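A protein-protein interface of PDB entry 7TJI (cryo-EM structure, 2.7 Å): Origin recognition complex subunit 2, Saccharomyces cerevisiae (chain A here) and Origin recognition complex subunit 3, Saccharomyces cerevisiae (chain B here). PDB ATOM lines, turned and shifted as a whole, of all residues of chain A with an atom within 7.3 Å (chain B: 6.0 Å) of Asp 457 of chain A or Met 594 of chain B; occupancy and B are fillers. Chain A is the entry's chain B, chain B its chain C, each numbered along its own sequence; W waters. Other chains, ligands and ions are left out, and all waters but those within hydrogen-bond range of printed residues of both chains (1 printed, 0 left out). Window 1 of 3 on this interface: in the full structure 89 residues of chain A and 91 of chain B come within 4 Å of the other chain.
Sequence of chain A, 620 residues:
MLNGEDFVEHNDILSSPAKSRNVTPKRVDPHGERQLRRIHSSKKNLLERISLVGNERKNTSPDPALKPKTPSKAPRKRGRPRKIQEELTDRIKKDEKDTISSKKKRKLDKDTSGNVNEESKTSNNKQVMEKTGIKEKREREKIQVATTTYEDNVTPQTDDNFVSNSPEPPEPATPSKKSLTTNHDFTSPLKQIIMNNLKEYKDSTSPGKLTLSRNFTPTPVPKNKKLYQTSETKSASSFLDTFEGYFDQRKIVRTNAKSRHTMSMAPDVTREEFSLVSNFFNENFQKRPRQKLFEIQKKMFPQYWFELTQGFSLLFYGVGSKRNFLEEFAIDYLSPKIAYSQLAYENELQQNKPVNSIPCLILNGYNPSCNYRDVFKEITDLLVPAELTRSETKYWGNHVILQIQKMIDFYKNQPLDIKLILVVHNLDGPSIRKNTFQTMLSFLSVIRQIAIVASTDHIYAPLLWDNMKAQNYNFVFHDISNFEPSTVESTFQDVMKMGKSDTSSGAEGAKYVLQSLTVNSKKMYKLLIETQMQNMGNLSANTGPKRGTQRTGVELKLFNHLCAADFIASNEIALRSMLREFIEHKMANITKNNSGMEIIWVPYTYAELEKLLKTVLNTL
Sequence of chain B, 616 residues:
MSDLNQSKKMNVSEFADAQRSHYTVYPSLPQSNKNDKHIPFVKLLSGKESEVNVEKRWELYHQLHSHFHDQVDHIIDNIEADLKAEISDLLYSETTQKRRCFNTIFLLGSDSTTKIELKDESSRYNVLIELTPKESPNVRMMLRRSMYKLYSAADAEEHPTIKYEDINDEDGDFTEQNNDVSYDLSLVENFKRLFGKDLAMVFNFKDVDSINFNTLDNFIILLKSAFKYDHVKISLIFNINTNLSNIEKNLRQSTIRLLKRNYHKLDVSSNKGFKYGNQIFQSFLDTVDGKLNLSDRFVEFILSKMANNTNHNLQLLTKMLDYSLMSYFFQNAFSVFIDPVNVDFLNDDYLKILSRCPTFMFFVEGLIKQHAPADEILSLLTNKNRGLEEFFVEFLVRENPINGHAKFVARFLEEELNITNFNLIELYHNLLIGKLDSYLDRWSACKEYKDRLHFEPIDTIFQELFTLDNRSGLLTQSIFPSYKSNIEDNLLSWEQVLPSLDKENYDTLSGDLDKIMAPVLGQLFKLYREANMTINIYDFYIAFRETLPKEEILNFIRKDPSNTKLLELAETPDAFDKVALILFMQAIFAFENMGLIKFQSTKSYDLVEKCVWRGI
The backbone NH (N) of Ile 459 of chain A sits at hydrogen-bond distance from the backbone carbonyl oxygen (O) of Met 594 of chain B. OH of Tyr 483 of chain B is in hydrogen-bond range of O of His 458 of chain A (2.8 Å). The side-chain hydroxyl of Thr 456 of chain A is in hydrogen-bond range of the side-chain hydroxyl of Tyr 483 of chain B.
The side-chain amino group (NZ) of Lys 322 of chain A sits at hydrogen-bond distance from the backbone carbonyl oxygen (O) of Gly 318 of chain A, at 3.0 Å. N of Asp 457 of chain A lies within hydrogen-bond range of OD2 of Asp 428 of chain A. OD1 of Asp 457 of chain A lies within salt-bridge range of NZ of Lys 322 of chain A (2.8 Å). ND1 of His 458 of chain A sits at hydrogen-bond distance from N of Tyr 460 of chain A (3.1 Å). OD2 of Asp 428 of chain A lies within hydrogen-bond range of N of His 458 of chain A (2.4 Å). O of Phe 316 of chain A is in hydrogen-bond range of N of Thr 456 of chain A (3.1 Å).
Among the printed residues, merely in contact across the chains: Tyr 317 of chain A with Tyr 483 of chain B (3.5 Å), Tyr 317 of chain A with Ile 487 of chain B (3.99 Å), Gly 318 of chain A with Ile 487 of chain B (3.7 Å), Val 319 of chain A with Ile 487 of chain B (3.99 Å), Val 319 of chain A with Leu 491 of chain B (3.7 Å), Val 319 of chain A with Met 594 of chain B (3.7 Å), Asp 457 of chain A with Met 594 of chain B (3.9 Å), His 458 of chain A with Asn 593 of chain B (3.7 Å), His 458 of chain A with Met 594 of chain B (3.3 Å), His 458 of chain A with Gly 595 of chain B (3.5 Å), Ile 459 of chain A with Tyr 483 of chain B (3.4 Å), Ile 459 of chain A with Ile 487 of chain B (3.7 Å), Ile 459 of chain A with Leu 596 of chain B (3.8 Å) and Ala 461 of chain A with Tyr 483 of chain B (3.6 Å).
Asp 457 of chain A touches just one residue of chain B: Met 594 (3.9 Å). Of chain A, only Val 319, Asp 457, His 458 and Ile 459 come within 4 Å of Met 594 of chain B. Printed residues of chain B within 4 Å of Ala 461 of chain A: Tyr 483 (3.6 Å). Of the printed residues of chain A, Asn 593 of chain B touches His 458 (3.7 Å). Of the printed residues of chain B, Tyr 317 of chain A touches Tyr 483 and Ile 487. The nearest printed residue of chain B that does not touch Asp 457 of chain A is Tyr 483 of chain B (4.5 Å). The nearest residue of chain A that does not touch Met 594 of chain B is Tyr 460 of chain A (5.0 Å). The nearest printed residue of chain A that does not touch Ile 487 of chain B is Asp 457 of chain A (6.0 Å).
Of the 21 printed residues of chain A, 8 touch a printed residue of chain B. Hydrophobic or aromatic side chains of chain A that line the printed part of chain B: Tyr 317, Val 319, His 458, Ile 459 and Ala 461. Of the 12 printed residues of chain B, 7 touch a printed residue of chain A. Printed residues of chain B that touch a printed residue of chain A: Tyr 483, Ile 487, Leu 491, Asn 593, Met 594, Gly 595 and Leu 596. Hydrophobic or aromatic side chains of chain B within 4 Å of the printed part of chain A: Tyr 483, Ile 487, Leu 491, Met 594 and Leu 596. Among the printed residues, no Asp or Glu carboxylate lies within 4 Å of a Lys or Arg side-chain nitrogen of the other chain.
Water W1 lies within hydrogen-bond range of O of Thr 456 of chain A, N of Gly 318 of chain A and OH of Tyr 483 of chain B.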
ATOM      1  N   PHE A 316     -10.561   2.719 -20.270  1.00  0.00           N
ATOM      2  CA  PHE A 316      -9.852   1.581 -20.818  1.00  0.00           C
ATOM      3  C   PHE A 316      -8.468   2.015 -21.273  1.00  0.00           C
ATOM      4  O   PHE A 316      -8.291   3.115 -21.795  1.00  0.00           O
ATOM      5  CB  PHE A 316     -10.633   0.974 -21.982  1.00  0.00           C
ATOM      6  CG  PHE A 316     -11.894   0.280 -21.562  1.00  0.00           C
ATOM      7  CD1 PHE A 316     -11.853  -0.997 -21.027  1.00  0.00           C
ATOM      8  CD2 PHE A 316     -13.124   0.907 -21.697  1.00  0.00           C
ATOM      9  CE1 PHE A 316     -13.012  -1.642 -20.638  1.00  0.00           C
ATOM     10  CE2 PHE A 316     -14.287   0.265 -21.308  1.00  0.00           C
ATOM     11  CZ  PHE A 316     -14.229  -1.011 -20.775  1.00  0.00           C
ATOM     12  N   TYR A 317      -7.485   1.158 -21.047  1.00  0.00           N
ATOM     13  CA  TYR A 317      -6.128   1.432 -21.483  1.00  0.00           C
ATOM     14  C   TYR A 317      -5.469   0.110 -21.838  1.00  0.00           C
ATOM     15  O   TYR A 317      -6.049  -0.963 -21.669  1.00  0.00           O
ATOM     16  CB  TYR A 317      -5.346   2.202 -20.415  1.00  0.00           C
ATOM     17  CG  TYR A 317      -4.976   1.393 -19.191  1.00  0.00           C
ATOM     18  CD1 TYR A 317      -5.905   1.154 -18.190  1.00  0.00           C
ATOM     19  CD2 TYR A 317      -3.696   0.867 -19.039  1.00  0.00           C
ATOM     20  CE1 TYR A 317      -5.579   0.415 -17.079  1.00  0.00           C
ATOM     21  CE2 TYR A 317      -3.360   0.122 -17.929  1.00  0.00           C
ATOM     22  CZ  TYR A 317      -4.305  -0.099 -16.952  1.00  0.00           C
ATOM     23  OH  TYR A 317      -3.980  -0.837 -15.842  1.00  0.00           O
ATOM     24  N   GLY A 318      -4.242   0.195 -22.329  1.00  0.00           N
ATOM     25  CA  GLY A 318      -3.533  -0.978 -22.788  1.00  0.00           C
ATOM     26  C   GLY A 318      -2.803  -0.688 -24.076  1.00  0.00           C
ATOM     27  O   GLY A 318      -2.942   0.405 -24.628  1.00  0.00           O
ATOM     28  N   VAL A 319      -2.027  -1.639 -24.570  1.00  0.00           N
ATOM     29  CA  VAL A 319      -1.298  -1.448 -25.817  1.00  0.00           C
ATOM     30  C   VAL A 319      -2.140  -1.990 -26.968  1.00  0.00           C
ATOM     31  O   VAL A 319      -2.723  -3.078 -26.880  1.00  0.00           O
ATOM     32  CB  VAL A 319       0.104  -2.088 -25.752  1.00  0.00           C
ATOM     33  CG1 VAL A 319       0.923  -1.379 -24.703  1.00  0.00           C
ATOM     34  CG2 VAL A 319       0.074  -3.573 -25.424  1.00  0.00           C
ATOM     35  N   GLY A 320      -2.268  -1.195 -28.017  1.00  0.00           N
ATOM     36  CA  GLY A 320      -3.124  -1.536 -29.131  1.00  0.00           C
ATOM     37  C   GLY A 320      -4.356  -0.648 -29.192  1.00  0.00           C
ATOM     38  O   GLY A 320      -4.720   0.040 -28.235  1.00  0.00           O
ATOM     39  N   SER A 321      -5.001  -0.666 -30.355  1.00  0.00           N
ATOM     40  CA  SER A 321      -6.184   0.154 -30.565  1.00  0.00           C
ATOM     41  C   SER A 321      -7.371  -0.404 -29.799  1.00  0.00           C
ATOM     42  O   SER A 321      -7.545  -1.618 -29.679  1.00  0.00           O
ATOM     43  CB  SER A 321      -6.529   0.235 -32.046  1.00  0.00           C
ATOM     44  OG  SER A 321      -7.651   1.074 -32.255  1.00  0.00           O
ATOM     45  N   LYS A 322      -8.191   0.500 -29.277  1.00  0.00           N
ATOM     46  CA  LYS A 322      -9.363   0.122 -28.504  1.00  0.00           C
ATOM     47  C   LYS A 322     -10.649   0.636 -29.140  1.00  0.00           C
ATOM     48  O   LYS A 322     -11.683   0.695 -28.472  1.00  0.00           O
ATOM     49  CB  LYS A 322      -9.223   0.625 -27.067  1.00  0.00           C
ATOM     50  CG  LYS A 322      -7.996   0.081 -26.356  1.00  0.00           C
ATOM     51  CD  LYS A 322      -7.687   0.846 -25.083  1.00  0.00           C
ATOM     52  CE  LYS A 322      -6.760   2.011 -25.347  1.00  0.00           C
ATOM     53  NZ  LYS A 322      -5.405   1.583 -25.782  1.00  0.00           N
ATOM     54  N   TYR A 366      -8.858  11.095 -31.464  1.00  0.00           N
ATOM     55  CA  TYR A 366      -7.673  11.013 -32.307  1.00  0.00           C
ATOM     56  C   TYR A 366      -7.716  12.005 -33.465  1.00  0.00           C
ATOM     57  O   TYR A 366      -6.671  12.275 -34.064  1.00  0.00           O
ATOM     58  CB  TYR A 366      -7.495   9.585 -32.836  1.00  0.00           C
ATOM     59  CG  TYR A 366      -8.694   9.008 -33.561  1.00  0.00           C
ATOM     60  CD1 TYR A 366      -9.681   8.307 -32.874  1.00  0.00           C
ATOM     61  CD2 TYR A 366      -8.822   9.137 -34.936  1.00  0.00           C
ATOM     62  CE1 TYR A 366     -10.767   7.778 -33.533  1.00  0.00           C
ATOM     63  CE2 TYR A 366      -9.906   8.611 -35.602  1.00  0.00           C
ATOM     64  CZ  TYR A 366     -10.875   7.934 -34.898  1.00  0.00           C
ATOM     65  OH  TYR A 366     -11.950   7.409 -35.568  1.00  0.00           O
ATOM     66  N   ASN A 426      -9.879   7.847 -27.399  1.00  0.00           N
ATOM     67  CA  ASN A 426      -8.652   8.626 -27.194  1.00  0.00           C
ATOM     68  C   ASN A 426      -8.931   9.914 -26.412  1.00  0.00           C
ATOM     69  O   ASN A 426      -8.836  11.015 -26.942  1.00  0.00           O
ATOM     70  CB  ASN A 426      -7.958   8.949 -28.525  1.00  0.00           C
ATOM     71  CG  ASN A 426      -7.323   7.738 -29.172  1.00  0.00           C
ATOM     72  OD1 ASN A 426      -6.103   7.600 -29.181  1.00  0.00           O
ATOM     73  ND2 ASN A 426      -8.144   6.867 -29.738  1.00  0.00           N
ATOM     74  N   LEU A 427      -9.293   9.738 -25.135  1.00  0.00           N
ATOM     75  CA  LEU A 427      -9.546  10.862 -24.228  1.00  0.00           C
ATOM     76  C   LEU A 427      -8.316  11.747 -24.026  1.00  0.00           C
ATOM     77  O   LEU A 427      -8.451  12.931 -23.705  1.00  0.00           O
ATOM     78  CB  LEU A 427     -10.040  10.321 -22.880  1.00  0.00           C
ATOM     79  CG  LEU A 427     -10.461  11.273 -21.757  1.00  0.00           C
ATOM     80  CD1 LEU A 427     -11.747  11.965 -22.114  1.00  0.00           C
ATOM     81  CD2 LEU A 427     -10.603  10.560 -20.435  1.00  0.00           C
ATOM     82  N   ASP A 428      -7.126  11.199 -24.227  1.00  0.00           N
ATOM     83  CA  ASP A 428      -5.861  11.904 -24.150  1.00  0.00           C
ATOM     84  C   ASP A 428      -5.393  12.433 -25.501  1.00  0.00           C
ATOM     85  O   ASP A 428      -4.246  12.872 -25.612  1.00  0.00           O
ATOM     86  CB  ASP A 428      -4.813  10.961 -23.577  1.00  0.00           C
ATOM     87  CG  ASP A 428      -4.773   9.652 -24.324  1.00  0.00           C
ATOM     88  OD1 ASP A 428      -5.774   9.328 -24.993  1.00  0.00           O
ATOM     89  OD2 ASP A 428      -3.745   8.958 -24.278  1.00  0.00           O
ATOM     90  N   GLY A 429      -6.246  12.382 -26.525  1.00  0.00           N
ATOM     91  CA  GLY A 429      -5.899  12.812 -27.862  1.00  0.00           C
ATOM     92  C   GLY A 429      -5.650  14.303 -27.964  1.00  0.00           C
ATOM     93  O   GLY A 429      -5.955  15.064 -27.040  1.00  0.00           O
ATOM     94  N   SER A 455     -11.271   5.920 -23.459  1.00  0.00           N
ATOM     95  CA  SER A 455     -10.010   5.210 -23.584  1.00  0.00           C
ATOM     96  C   SER A 455      -8.864   6.210 -23.652  1.00  0.00           C
ATOM     97  O   SER A 455      -9.052   7.363 -24.041  1.00  0.00           O
ATOM     98  CB  SER A 455      -9.987   4.302 -24.817  1.00  0.00           C
ATOM     99  OG  SER A 455      -9.878   5.055 -26.010  1.00  0.00           O
ATOM    100  N   THR A 456      -7.675   5.760 -23.254  1.00  0.00           N
ATOM    101  CA  THR A 456      -6.465   6.564 -23.337  1.00  0.00           C
ATOM    102  C   THR A 456      -5.348   5.746 -23.968  1.00  0.00           C
ATOM    103  O   THR A 456      -5.296   4.525 -23.824  1.00  0.00           O
ATOM    104  CB  THR A 456      -6.005   7.080 -21.958  1.00  0.00           C
ATOM    105  OG1 THR A 456      -5.994   6.003 -21.015  1.00  0.00           O
ATOM    106  CG2 THR A 456      -6.925   8.194 -21.452  1.00  0.00           C
ATOM    107  N   ASP A 457      -4.445   6.436 -24.660  1.00  0.00           N
ATOM    108  CA  ASP A 457      -3.323   5.793 -25.331  1.00  0.00           C
ATOM    109  C   ASP A 457      -1.958   6.252 -24.843  1.00  0.00           C
ATOM    110  O   ASP A 457      -1.012   5.464 -24.885  1.00  0.00           O
ATOM    111  CB  ASP A 457      -3.403   6.025 -26.846  1.00  0.00           C
ATOM    112  CG  ASP A 457      -3.998   4.848 -27.581  1.00  0.00           C
ATOM    113  OD1 ASP A 457      -4.062   3.753 -26.987  1.00  0.00           O
ATOM    114  OD2 ASP A 457      -4.398   5.015 -28.751  1.00  0.00           O
ATOM    115  N   HIS A 458      -1.829   7.494 -24.382  1.00  0.00           N
ATOM    116  CA  HIS A 458      -0.537   8.006 -23.947  1.00  0.00           C
ATOM    117  C   HIS A 458      -0.153   7.419 -22.596  1.00  0.00           C
ATOM    118  O   HIS A 458      -1.000   7.231 -21.721  1.00  0.00           O
ATOM    119  CB  HIS A 458      -0.575   9.528 -23.865  1.00  0.00           C
ATOM    120  CG  HIS A 458       0.764  10.179 -24.015  1.00  0.00           C
ATOM    121  ND1 HIS A 458       1.646  10.317 -22.966  1.00  0.00           N
ATOM    122  CD2 HIS A 458       1.364  10.741 -25.088  1.00  0.00           C
ATOM    123  CE1 HIS A 458       2.737  10.928 -23.391  1.00  0.00           C
ATOM    124  NE2 HIS A 458       2.589  11.198 -24.674  1.00  0.00           N
ATOM    125  N   ILE A 459       1.141   7.137 -22.427  1.00  0.00           N
ATOM    126  CA  ILE A 459       1.625   6.529 -21.191  1.00  0.00           C
ATOM    127  C   ILE A 459       1.614   7.516 -20.024  1.00  0.00           C
ATOM    128  O   ILE A 459       1.674   7.098 -18.864  1.00  0.00           O
ATOM    129  CB  ILE A 459       3.029   5.925 -21.420  1.00  0.00           C
ATOM    130  CG1 ILE A 459       3.273   4.753 -20.468  1.00  0.00           C
ATOM    131  CG2 ILE A 459       4.125   6.976 -21.285  1.00  0.00           C
ATOM    132  CD1 ILE A 459       4.481   3.947 -20.779  1.00  0.00           C
ATOM    133  N   TYR A 460       1.519   8.815 -20.300  1.00  0.00           N
ATOM    134  CA  TYR A 460       1.481   9.852 -19.279  1.00  0.00           C
ATOM    135  C   TYR A 460       0.083  10.411 -19.063  1.00  0.00           C
ATOM    136  O   TYR A 460      -0.048  11.468 -18.442  1.00  0.00           O
ATOM    137  CB  TYR A 460       2.424  10.993 -19.657  1.00  0.00           C
ATOM    138  CG  TYR A 460       3.875  10.778 -19.311  1.00  0.00           C
ATOM    139  CD1 TYR A 460       4.296   9.639 -18.637  1.00  0.00           C
ATOM    140  CD2 TYR A 460       4.832  11.705 -19.700  1.00  0.00           C
ATOM    141  CE1 TYR A 460       5.628   9.446 -18.338  1.00  0.00           C
ATOM    142  CE2 TYR A 460       6.163  11.517 -19.414  1.00  0.00           C
ATOM    143  CZ  TYR A 460       6.557  10.389 -18.730  1.00  0.00           C
ATOM    144  OH  TYR A 460       7.891  10.217 -18.448  1.00  0.00           O
ATOM    145  N   ALA A 461      -0.945   9.744 -19.589  1.00  0.00           N
ATOM    146  CA  ALA A 461      -2.333  10.208 -19.493  1.00  0.00           C
ATOM    147  C   ALA A 461      -2.869  10.520 -18.086  1.00  0.00           C
ATOM    148  O   ALA A 461      -3.601  11.519 -17.964  1.00  0.00           O
ATOM    149  CB  ALA A 461      -3.251   9.195 -20.197  1.00  0.00           C
ATOM    150  N   SER A 486      -4.015  -0.077 -34.845  1.00  0.00           N
ATOM    151  CA  SER A 486      -4.450   1.327 -34.838  1.00  0.00           C
ATOM    152  C   SER A 486      -4.441   1.926 -36.248  1.00  0.00           C
ATOM    153  O   SER A 486      -3.796   2.939 -36.525  1.00  0.00           O
ATOM    154  CB  SER A 486      -3.618   2.166 -33.854  1.00  0.00           C
ATOM    155  OG  SER A 486      -4.136   3.475 -33.718  1.00  0.00           O
ATOM    156  N   GLU A 489      -6.646   5.494 -36.454  1.00  0.00           N
ATOM    157  CA  GLU A 489      -5.993   6.626 -35.806  1.00  0.00           C
ATOM    158  C   GLU A 489      -4.675   7.009 -36.470  1.00  0.00           C
ATOM    159  O   GLU A 489      -4.200   8.130 -36.268  1.00  0.00           O
ATOM    160  CB  GLU A 489      -5.755   6.318 -34.327  1.00  0.00           C
ATOM    161  CG  GLU A 489      -7.006   5.936 -33.552  1.00  0.00           C
ATOM    162  CD  GLU A 489      -7.102   4.447 -33.281  1.00  0.00           C
ATOM    163  OE1 GLU A 489      -7.380   3.683 -34.229  1.00  0.00           O
ATOM    164  OE2 GLU A 489      -6.900   4.042 -32.119  1.00  0.00           O
ATOM    165  N   TYR B 483      -0.317   2.236 -13.824  1.00  0.00           N
ATOM    166  CA  TYR B 483      -0.783   2.352 -15.204  1.00  0.00           C
ATOM    167  C   TYR B 483       0.364   2.210 -16.196  1.00  0.00           C
ATOM    168  O   TYR B 483       0.350   1.337 -17.082  1.00  0.00           O
ATOM    169  CB  TYR B 483      -1.492   3.709 -15.346  1.00  0.00           C
ATOM    170  CG  TYR B 483      -1.868   4.200 -16.729  1.00  0.00           C
ATOM    171  CD1 TYR B 483      -0.972   4.937 -17.505  1.00  0.00           C
ATOM    172  CD2 TYR B 483      -3.143   3.999 -17.227  1.00  0.00           C
ATOM    173  CE1 TYR B 483      -1.320   5.398 -18.757  1.00  0.00           C
ATOM    174  CE2 TYR B 483      -3.502   4.474 -18.472  1.00  0.00           C
ATOM    175  CZ  TYR B 483      -2.587   5.166 -19.235  1.00  0.00           C
ATOM    176  OH  TYR B 483      -2.942   5.635 -20.478  1.00  0.00           O
ATOM    177  N   ILE B 487       1.595  -0.921 -18.741  1.00  0.00           N
ATOM    178  CA  ILE B 487       1.911  -0.734 -20.162  1.00  0.00           C
ATOM    179  C   ILE B 487       3.292  -1.305 -20.490  1.00  0.00           C
ATOM    180  O   ILE B 487       3.458  -2.100 -21.428  1.00  0.00           O
ATOM    181  CB  ILE B 487       1.832   0.761 -20.525  1.00  0.00           C
ATOM    182  CG1 ILE B 487       0.392   1.264 -20.457  1.00  0.00           C
ATOM    183  CG2 ILE B 487       2.429   1.015 -21.894  1.00  0.00           C
ATOM    184  CD1 ILE B 487      -0.516   0.603 -21.436  1.00  0.00           C
ATOM    185  N   LEU B 491       4.257  -4.659 -22.704  1.00  0.00           N
ATOM    186  CA  LEU B 491       5.109  -4.506 -23.882  1.00  0.00           C
ATOM    187  C   LEU B 491       6.377  -5.346 -23.784  1.00  0.00           C
ATOM    188  O   LEU B 491       6.814  -5.928 -24.782  1.00  0.00           O
ATOM    189  CB  LEU B 491       5.469  -3.037 -24.090  1.00  0.00           C
ATOM    190  CG  LEU B 491       4.547  -2.248 -25.020  1.00  0.00           C
ATOM    191  CD1 LEU B 491       5.080  -0.848 -25.240  1.00  0.00           C
ATOM    192  CD2 LEU B 491       4.339  -2.971 -26.343  1.00  0.00           C
ATOM    193  N   LEU B 521       5.367  -4.372 -31.777  1.00  0.00           N
ATOM    194  CA  LEU B 521       5.563  -3.412 -30.694  1.00  0.00           C
ATOM    195  C   LEU B 521       6.359  -4.022 -29.547  1.00  0.00           C
ATOM    196  O   LEU B 521       7.287  -3.392 -29.027  1.00  0.00           O
ATOM    197  CB  LEU B 521       4.214  -2.909 -30.184  1.00  0.00           C
ATOM    198  CG  LEU B 521       3.360  -2.016 -31.078  1.00  0.00           C
ATOM    199  CD1 LEU B 521       2.182  -1.476 -30.290  1.00  0.00           C
ATOM    200  CD2 LEU B 521       4.179  -0.886 -31.636  1.00  0.00           C
ATOM    201  N   PHE B 589       5.978   5.096 -35.214  1.00  0.00           N
ATOM    202  CA  PHE B 589       4.952   6.108 -34.946  1.00  0.00           C
ATOM    203  C   PHE B 589       3.857   5.640 -33.986  1.00  0.00           C
ATOM    204  O   PHE B 589       3.243   6.497 -33.336  1.00  0.00           O
ATOM    205  CB  PHE B 589       4.334   6.717 -36.220  1.00  0.00           C
ATOM    206  CG  PHE B 589       5.338   7.360 -37.161  1.00  0.00           C
ATOM    207  CD1 PHE B 589       6.128   6.624 -38.020  1.00  0.00           C
ATOM    208  CD2 PHE B 589       5.499   8.740 -37.141  1.00  0.00           C
ATOM    209  CE1 PHE B 589       7.038   7.238 -38.858  1.00  0.00           C
ATOM    210  CE2 PHE B 589       6.410   9.364 -37.973  1.00  0.00           C
ATOM    211  CZ  PHE B 589       7.182   8.609 -38.833  1.00  0.00           C
ATOM    212  N   ALA B 590       3.650   4.330 -33.798  1.00  0.00           N
ATOM    213  CA  ALA B 590       2.822   3.887 -32.674  1.00  0.00           C
ATOM    214  C   ALA B 590       3.450   4.266 -31.333  1.00  0.00           C
ATOM    215  O   ALA B 590       2.760   4.757 -30.430  1.00  0.00           O
ATOM    216  CB  ALA B 590       2.595   2.378 -32.752  1.00  0.00           C
ATOM    217  N   PHE B 591       4.768   4.075 -31.206  1.00  0.00           N
ATOM    218  CA  PHE B 591       5.492   4.484 -30.002  1.00  0.00           C
ATOM    219  C   PHE B 591       5.469   6.000 -29.824  1.00  0.00           C
ATOM    220  O   PHE B 591       5.401   6.499 -28.697  1.00  0.00           O
ATOM    221  CB  PHE B 591       6.941   3.992 -30.064  1.00  0.00           C
ATOM    222  CG  PHE B 591       7.139   2.567 -29.603  1.00  0.00           C
ATOM    223  CD1 PHE B 591       6.063   1.715 -29.398  1.00  0.00           C
ATOM    224  CD2 PHE B 591       8.420   2.081 -29.394  1.00  0.00           C
ATOM    225  CE1 PHE B 591       6.263   0.414 -28.983  1.00  0.00           C
ATOM    226  CE2 PHE B 591       8.625   0.779 -28.980  1.00  0.00           C
ATOM    227  CZ  PHE B 591       7.546  -0.054 -28.778  1.00  0.00           C
ATOM    228  N   GLU B 592       5.541   6.743 -30.933  1.00  0.00           N
ATOM    229  CA  GLU B 592       5.476   8.204 -30.881  1.00  0.00           C
ATOM    230  C   GLU B 592       4.117   8.679 -30.377  1.00  0.00           C
ATOM    231  O   GLU B 592       4.038   9.635 -29.598  1.00  0.00           O
ATOM    232  CB  GLU B 592       5.805   8.780 -32.268  1.00  0.00           C
ATOM    233  CG  GLU B 592       5.642  10.303 -32.525  1.00  0.00           C
ATOM    234  CD  GLU B 592       4.210  10.763 -32.801  1.00  0.00           C
ATOM    235  OE1 GLU B 592       3.608  10.289 -33.787  1.00  0.00           O
ATOM    236  OE2 GLU B 592       3.688  11.589 -32.022  1.00  0.00           O
ATOM    237  N   ASN B 593       3.038   8.040 -30.834  1.00  0.00           N
ATOM    238  CA  ASN B 593       1.715   8.387 -30.329  1.00  0.00           C
ATOM    239  C   ASN B 593       1.545   7.976 -28.872  1.00  0.00           C
ATOM    240  O   ASN B 593       0.849   8.657 -28.112  1.00  0.00           O
ATOM    241  CB  ASN B 593       0.632   7.740 -31.190  1.00  0.00           C
ATOM    242  CG  ASN B 593      -0.622   8.585 -31.272  1.00  0.00           C
ATOM    243  OD1 ASN B 593      -0.631   9.643 -31.899  1.00  0.00           O
ATOM    244  ND2 ASN B 593      -1.688   8.127 -30.628  1.00  0.00           N
ATOM    245  N   MET B 594       2.175   6.870 -28.467  1.00  0.00           N
ATOM    246  CA  MET B 594       2.102   6.445 -27.073  1.00  0.00           C
ATOM    247  C   MET B 594       2.912   7.351 -26.154  1.00  0.00           C
ATOM    248  O   MET B 594       2.595   7.470 -24.967  1.00  0.00           O
ATOM    249  CB  MET B 594       2.589   5.009 -26.950  1.00  0.00           C
ATOM    250  CG  MET B 594       1.570   3.982 -27.362  1.00  0.00           C
ATOM    251  SD  MET B 594       2.233   2.332 -27.133  1.00  0.00           S
ATOM    252  CE  MET B 594       1.883   2.124 -25.401  1.00  0.00           C
ATOM    253  N   GLY B 595       3.962   7.977 -26.671  1.00  0.00           N
ATOM    254  CA  GLY B 595       4.814   8.824 -25.870  1.00  0.00           C
ATOM    255  C   GLY B 595       6.098   8.186 -25.395  1.00  0.00           C
ATOM    256  O   GLY B 595       6.749   8.744 -24.508  1.00  0.00           O
ATOM    257  N   LEU B 596       6.474   7.029 -25.945  1.00  0.00           N
ATOM    258  CA  LEU B 596       7.729   6.389 -25.565  1.00  0.00           C
ATOM    259  C   LEU B 596       8.936   7.108 -26.161  1.00  0.00           C
ATOM    260  O   LEU B 596       9.951   7.282 -25.480  1.00  0.00           O
ATOM    261  CB  LEU B 596       7.726   4.918 -25.986  1.00  0.00           C
ATOM    262  CG  LEU B 596       6.583   4.001 -25.541  1.00  0.00           C
ATOM    263  CD1 LEU B 596       6.921   2.555 -25.834  1.00  0.00           C
ATOM    264  CD2 LEU B 596       6.277   4.164 -24.075  1.00  0.00           C
HETATM  265  O   HOH W   1      -3.008   3.090 -22.871  1.00  0.00           O
